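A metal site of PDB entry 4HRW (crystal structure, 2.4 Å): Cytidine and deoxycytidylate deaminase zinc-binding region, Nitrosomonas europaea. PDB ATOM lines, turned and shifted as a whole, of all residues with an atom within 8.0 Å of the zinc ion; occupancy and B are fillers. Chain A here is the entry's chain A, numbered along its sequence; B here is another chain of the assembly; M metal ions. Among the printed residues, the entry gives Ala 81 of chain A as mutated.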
ATOM      1  N   PHE A  50      16.880   5.517  -0.031  1.00  0.00           N
ATOM      2  CA  PHE A  50      16.449   5.660  -1.407  1.00  0.00           C
ATOM      3  C   PHE A  50      15.469   4.568  -1.787  1.00  0.00           C
ATOM      4  O   PHE A  50      15.593   3.420  -1.349  1.00  0.00           O
ATOM      5  CB  PHE A  50      17.646   5.575  -2.358  1.00  0.00           C
ATOM      6  CG  PHE A  50      18.663   6.666  -2.167  1.00  0.00           C
ATOM      7  CD1 PHE A  50      18.444   7.930  -2.692  1.00  0.00           C
ATOM      8  CD2 PHE A  50      19.852   6.415  -1.500  1.00  0.00           C
ATOM      9  CE1 PHE A  50      19.403   8.940  -2.558  1.00  0.00           C
ATOM     10  CE2 PHE A  50      20.817   7.408  -1.364  1.00  0.00           C
ATOM     11  CZ  PHE A  50      20.587   8.668  -1.897  1.00  0.00           C
ATOM     12  N   ASN A  68      17.394   0.962  -2.204  1.00  0.00           N
ATOM     13  CA  ASN A  68      18.839   0.838  -2.139  1.00  0.00           C
ATOM     14  C   ASN A  68      19.204  -0.346  -1.227  1.00  0.00           C
ATOM     15  O   ASN A  68      18.838  -0.369  -0.059  1.00  0.00           O
ATOM     16  CB  ASN A  68      19.445   2.123  -1.573  1.00  0.00           C
ATOM     17  CG  ASN A  68      20.952   2.064  -1.449  1.00  0.00           C
ATOM     18  OD1 ASN A  68      21.681   2.573  -2.297  1.00  0.00           O
ATOM     19  ND2 ASN A  68      21.429   1.442  -0.396  1.00  0.00           N
ATOM     20  N   VAL A  70      22.555  -1.674  -1.570  1.00  0.00           N
ATOM     21  CA  VAL A  70      23.992  -1.747  -1.793  1.00  0.00           C
ATOM     22  C   VAL A  70      24.789  -2.499  -0.708  1.00  0.00           C
ATOM     23  O   VAL A  70      25.456  -3.505  -1.001  1.00  0.00           O
ATOM     24  CB  VAL A  70      24.582  -0.319  -1.949  1.00  0.00           C
ATOM     25  CG1 VAL A  70      26.107  -0.354  -1.874  1.00  0.00           C
ATOM     26  CG2 VAL A  70      24.144   0.264  -3.288  1.00  0.00           C
ATOM     27  N   SER A  76      27.226  -2.804  -5.310  1.00  0.00           N
ATOM     28  CA  SER A  76      27.141  -1.358  -5.505  1.00  0.00           C
ATOM     29  C   SER A  76      26.178  -0.974  -6.613  1.00  0.00           C
ATOM     30  O   SER A  76      25.784   0.192  -6.737  1.00  0.00           O
ATOM     31  CB  SER A  76      28.532  -0.765  -5.795  1.00  0.00           C
ATOM     32  OG  SER A  76      29.126  -1.349  -6.939  1.00  0.00           O
ATOM     33  N   ALA A  77      25.773  -1.941  -7.421  1.00  0.00           N
ATOM     34  CA  ALA A  77      24.830  -1.663  -8.492  1.00  0.00           C
ATOM     35  C   ALA A  77      23.385  -1.692  -7.971  1.00  0.00           C
ATOM     36  O   ALA A  77      22.451  -1.350  -8.697  1.00  0.00           O
ATOM     37  CB  ALA A  77      24.989  -2.680  -9.618  1.00  0.00           C
ATOM     38  N   ALA A  78      23.215  -2.092  -6.718  1.00  0.00           N
ATOM     39  CA  ALA A  78      21.887  -2.191  -6.125  1.00  0.00           C
ATOM     40  C   ALA A  78      21.244  -0.887  -5.669  1.00  0.00           C
ATOM     41  O   ALA A  78      20.947  -0.710  -4.492  1.00  0.00           O
ATOM     42  CB  ALA A  78      21.895  -3.195  -4.981  1.00  0.00           C
ATOM     43  N   HIS A  79      21.011   0.025  -6.609  1.00  0.00           N
ATOM     44  CA  HIS A  79      20.358   1.288  -6.308  1.00  0.00           C
ATOM     45  C   HIS A  79      18.861   1.110  -6.496  1.00  0.00           C
ATOM     46  O   HIS A  79      18.421   0.180  -7.174  1.00  0.00           O
ATOM     47  CB  HIS A  79      20.851   2.386  -7.237  1.00  0.00           C
ATOM     48  CG  HIS A  79      22.207   2.905  -6.892  1.00  0.00           C
ATOM     49  ND1 HIS A  79      22.655   4.132  -7.306  1.00  0.00           N
ATOM     50  CD2 HIS A  79      23.223   2.344  -6.188  1.00  0.00           C
ATOM     51  CE1 HIS A  79      23.894   4.320  -6.867  1.00  0.00           C
ATOM     52  NE2 HIS A  79      24.255   3.247  -6.190  1.00  0.00           N
ATOM     53  N   ALA A  80      18.078   1.997  -5.886  1.00  0.00           N
ATOM     54  CA  ALA A  80      16.628   1.920  -5.961  1.00  0.00           C
ATOM     55  C   ALA A  80      16.076   1.826  -7.384  1.00  0.00           C
ATOM     56  O   ALA A  80      15.328   0.907  -7.716  1.00  0.00           O
ATOM     57  CB  ALA A  80      16.003   3.114  -5.241  1.00  0.00           C
ATOM     58  N   ALA A  81      16.465   2.788  -8.229  1.00  0.00           N
ATOM     59  CA  ALA A  81      15.986   2.814  -9.609  1.00  0.00           C
ATOM     60  C   ALA A  81      16.299   1.525 -10.355  1.00  0.00           C
ATOM     61  O   ALA A  81      15.455   1.011 -11.098  1.00  0.00           O
ATOM     62  CB  ALA A  81      16.599   4.017 -10.340  1.00  0.00           C
ATOM     63  N   ILE A  82      17.498   0.993 -10.168  1.00  0.00           N
ATOM     64  CA  ILE A  82      17.864  -0.224 -10.870  1.00  0.00           C
ATOM     65  C   ILE A  82      17.092  -1.460 -10.417  1.00  0.00           C
ATOM     66  O   ILE A  82      16.686  -2.273 -11.248  1.00  0.00           O
ATOM     67  CB  ILE A  82      19.410  -0.481 -10.794  1.00  0.00           C
ATOM     68  CG1 ILE A  82      20.073   0.342 -11.903  1.00  0.00           C
ATOM     69  CG2 ILE A  82      19.735  -1.972 -10.921  1.00  0.00           C
ATOM     70  CD1 ILE A  82      21.512  -0.027 -12.201  1.00  0.00           C
ATOM     71  N   THR A 109      10.983   7.931  -8.399  1.00  0.00           N
ATOM     72  CA  THR A 109      12.127   7.802  -7.502  1.00  0.00           C
ATOM     73  C   THR A 109      12.251   8.927  -6.469  1.00  0.00           C
ATOM     74  O   THR A 109      12.010  10.090  -6.776  1.00  0.00           O
ATOM     75  CB  THR A 109      13.415   7.719  -8.316  1.00  0.00           C
ATOM     76  OG1 THR A 109      14.520   7.456  -7.451  1.00  0.00           O
ATOM     77  CG2 THR A 109      13.646   9.036  -9.063  1.00  0.00           C
ATOM     78  N   ALA A 111      14.808  10.287  -5.201  1.00  0.00           N
ATOM     79  CA  ALA A 111      15.891  11.230  -5.457  1.00  0.00           C
ATOM     80  C   ALA A 111      16.305  11.182  -6.922  1.00  0.00           C
ATOM     81  O   ALA A 111      16.203  10.134  -7.560  1.00  0.00           O
ATOM     82  CB  ALA A 111      17.094  10.913  -4.564  1.00  0.00           C
ATOM     83  N   GLU A 112      16.742  12.317  -7.453  1.00  0.00           N
ATOM     84  CA  GLU A 112      17.177  12.340  -8.842  1.00  0.00           C
ATOM     85  C   GLU A 112      18.248  11.277  -9.028  1.00  0.00           C
ATOM     86  O   GLU A 112      19.129  11.104  -8.197  1.00  0.00           O
ATOM     87  CB  GLU A 112      17.705  13.732  -9.208  1.00  0.00           C
ATOM     88  CG  GLU A 112      16.642  14.803  -9.101  1.00  0.00           C
ATOM     89  CD  GLU A 112      17.085  16.151  -9.629  1.00  0.00           C
ATOM     90  OE1 GLU A 112      18.250  16.545  -9.424  1.00  0.00           O
ATOM     91  OE2 GLU A 112      16.236  16.821 -10.252  1.00  0.00           O
ATOM     92  N   PRO A 113      18.168  10.542 -10.144  1.00  0.00           N
ATOM     93  CA  PRO A 113      19.124   9.471 -10.455  1.00  0.00           C
ATOM     94  C   PRO A 113      20.581   9.881 -10.649  1.00  0.00           C
ATOM     95  O   PRO A 113      20.875  10.889 -11.285  1.00  0.00           O
ATOM     96  CB  PRO A 113      18.529   8.857 -11.708  1.00  0.00           C
ATOM     97  CG  PRO A 113      17.996  10.082 -12.419  1.00  0.00           C
ATOM     98  CD  PRO A 113      17.264  10.777 -11.287  1.00  0.00           C
ATOM     99  N   CYS A 114      21.476   9.061 -10.105  1.00  0.00           N
ATOM    100  CA  CYS A 114      22.907   9.287 -10.261  1.00  0.00           C
ATOM    101  C   CYS A 114      23.209   8.918 -11.718  1.00  0.00           C
ATOM    102  O   CYS A 114      22.309   8.527 -12.467  1.00  0.00           O
ATOM    103  CB  CYS A 114      23.697   8.364  -9.323  1.00  0.00           C
ATOM    104  SG  CYS A 114      23.798   6.624  -9.849  1.00  0.00           S
ATOM    105  N   VAL A 115      24.461   9.035 -12.128  1.00  0.00           N
ATOM    106  CA  VAL A 115      24.824   8.745 -13.506  1.00  0.00           C
ATOM    107  C   VAL A 115      24.522   7.301 -13.904  1.00  0.00           C
ATOM    108  O   VAL A 115      24.002   7.047 -14.994  1.00  0.00           O
ATOM    109  CB  VAL A 115      26.302   9.114 -13.759  1.00  0.00           C
ATOM    110  CG1 VAL A 115      27.202   8.358 -12.777  1.00  0.00           C
ATOM    111  CG2 VAL A 115      26.671   8.806 -15.213  1.00  0.00           C
ATOM    112  N   MET A 116      24.821   6.350 -13.013  1.00  0.00           N
ATOM    113  CA  MET A 116      24.546   4.947 -13.304  1.00  0.00           C
ATOM    114  C   MET A 116      23.047   4.694 -13.579  1.00  0.00           C
ATOM    115  O   MET A 116      22.673   4.182 -14.646  1.00  0.00           O
ATOM    116  CB  MET A 116      24.989   4.080 -12.126  1.00  0.00           C
ATOM    117  CG  MET A 116      24.453   2.665 -12.200  1.00  0.00           C
ATOM    118  SD  MET A 116      24.808   1.747 -10.700  1.00  0.00           S
ATOM    119  CE  MET A 116      25.621   0.362 -11.390  1.00  0.00           C
ATOM    120  N   CYS A 117      22.215   5.063 -12.616  1.00  0.00           N
ATOM    121  CA  CYS A 117      20.770   4.893 -12.742  1.00  0.00           C
ATOM    122  C   CYS A 117      20.218   5.744 -13.887  1.00  0.00           C
ATOM    123  O   CYS A 117      19.225   5.386 -14.512  1.00  0.00           O
ATOM    124  CB  CYS A 117      20.090   5.247 -11.407  1.00  0.00           C
ATOM    125  SG  CYS A 117      20.510   4.062 -10.070  1.00  0.00           S
ATOM    126  N   PHE A 118      20.876   6.875 -14.147  1.00  0.00           N
ATOM    127  CA  PHE A 118      20.495   7.755 -15.241  1.00  0.00           C
ATOM    128  C   PHE A 118      20.493   6.908 -16.514  1.00  0.00           C
ATOM    129  O   PHE A 118      19.488   6.845 -17.237  1.00  0.00           O
ATOM    130  CB  PHE A 118      21.523   8.894 -15.365  1.00  0.00           C
ATOM    131  CG  PHE A 118      21.470   9.629 -16.682  1.00  0.00           C
ATOM    132  CD1 PHE A 118      20.319  10.306 -17.078  1.00  0.00           C
ATOM    133  CD2 PHE A 118      22.575   9.630 -17.533  1.00  0.00           C
ATOM    134  CE1 PHE A 118      20.267  10.962 -18.283  1.00  0.00           C
ATOM    135  CE2 PHE A 118      22.524  10.285 -18.752  1.00  0.00           C
ATOM    136  CZ  PHE A 118      21.376  10.958 -19.127  1.00  0.00           C
ATOM    137  N   GLY A 119      21.614   6.242 -16.783  1.00  0.00           N
ATOM    138  CA  GLY A 119      21.700   5.387 -17.947  1.00  0.00           C
ATOM    139  C   GLY A 119      20.715   4.228 -17.861  1.00  0.00           C
ATOM    140  O   GLY A 119      20.155   3.812 -18.881  1.00  0.00           O
ATOM    141  N   ALA A 120      20.508   3.703 -16.661  1.00  0.00           N
ATOM    142  CA  ALA A 120      19.586   2.592 -16.436  1.00  0.00           C
ATOM    143  C   ALA A 120      18.178   2.963 -16.883  1.00  0.00           C
ATOM    144  O   ALA A 120      17.461   2.139 -17.466  1.00  0.00           O
ATOM    145  CB  ALA A 120      19.575   2.226 -14.956  1.00  0.00           C
ATOM    146  N   ASP A 144      27.218  10.850  -3.601  1.00  0.00           N
ATOM    147  CA  ASP A 144      27.662  11.391  -4.885  1.00  0.00           C
ATOM    148  C   ASP A 144      26.758  10.934  -6.036  1.00  0.00           C
ATOM    149  O   ASP A 144      26.482   9.747  -6.191  1.00  0.00           O
ATOM    150  CB  ASP A 144      29.100  10.945  -5.171  1.00  0.00           C
ATOM    151  CG  ASP A 144      29.788  11.799  -6.215  1.00  0.00           C
ATOM    152  OD1 ASP A 144      29.191  12.042  -7.285  1.00  0.00           O
ATOM    153  OD2 ASP A 144      30.933  12.220  -5.970  1.00  0.00           O
ATOM    154  N   GLU A 145      26.336  11.892  -6.861  1.00  0.00           N
ATOM    155  CA  GLU A 145      25.488  11.595  -8.002  1.00  0.00           C
ATOM    156  C   GLU A 145      26.324  11.152  -9.210  1.00  0.00           C
ATOM    157  O   GLU A 145      25.799  10.565 -10.159  1.00  0.00           O
ATOM    158  CB  GLU A 145      24.645  12.819  -8.359  1.00  0.00           C
ATOM    159  CG  GLU A 145      23.623  13.210  -7.295  1.00  0.00           C
ATOM    160  CD  GLU A 145      22.414  12.282  -7.273  1.00  0.00           C
ATOM    161  OE1 GLU A 145      22.596  11.055  -7.167  1.00  0.00           O
ATOM    162  OE2 GLU A 145      21.271  12.792  -7.339  1.00  0.00           O
ATOM    163  N   TRP B 123      31.217   3.312  -9.071  1.00  0.00           N
ATOM    164  CA  TRP B 123      30.782   2.904  -7.737  1.00  0.00           C
ATOM    165  C   TRP B 123      31.289   1.526  -7.304  1.00  0.00           C
ATOM    166  O   TRP B 123      31.130   1.156  -6.145  1.00  0.00           O
ATOM    167  CB  TRP B 123      29.243   2.870  -7.659  1.00  0.00           C
ATOM    168  CG  TRP B 123      28.522   4.101  -8.125  1.00  0.00           C
ATOM    169  CD1 TRP B 123      27.421   4.142  -8.927  1.00  0.00           C
ATOM    170  CD2 TRP B 123      28.866   5.462  -7.846  1.00  0.00           C
ATOM    171  NE1 TRP B 123      27.058   5.439  -9.170  1.00  0.00           N
ATOM    172  CE2 TRP B 123      27.925   6.270  -8.522  1.00  0.00           C
ATOM    173  CE3 TRP B 123      29.877   6.071  -7.092  1.00  0.00           C
ATOM    174  CZ2 TRP B 123      27.968   7.671  -8.460  1.00  0.00           C
ATOM    175  CZ3 TRP B 123      29.914   7.465  -7.030  1.00  0.00           C
ATOM    176  CH2 TRP B 123      28.961   8.245  -7.713  1.00  0.00           C
HETATM  177 ZN    ZN M   1      21.952   5.472  -8.852  1.00  0.00          ZN
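A ring nitrogen (NE2) of His 79 sits close to the backbone carbonyl oxygen (O) of Ser 76. The side-chain sulfur (SG) of Cys 114 lies close to the backbone NH (N) of Met 116, 3.3 Å away. The indole nitrogen (NE1) of Trp 123 of chain B sits close to the side-chain sulfur (SG) of Cys 114, 3.5 Å away.
The zinc ion is bound by a ring nitrogen (ND1) of His 79 (2.2 Å), the side-chain sulfur of Cys 117 (2.4 Å) and the side-chain sulfur of Cys 114 (2.4 Å).
Of the 24 residues printed, 3 come within 4 Å of the zinc ion.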
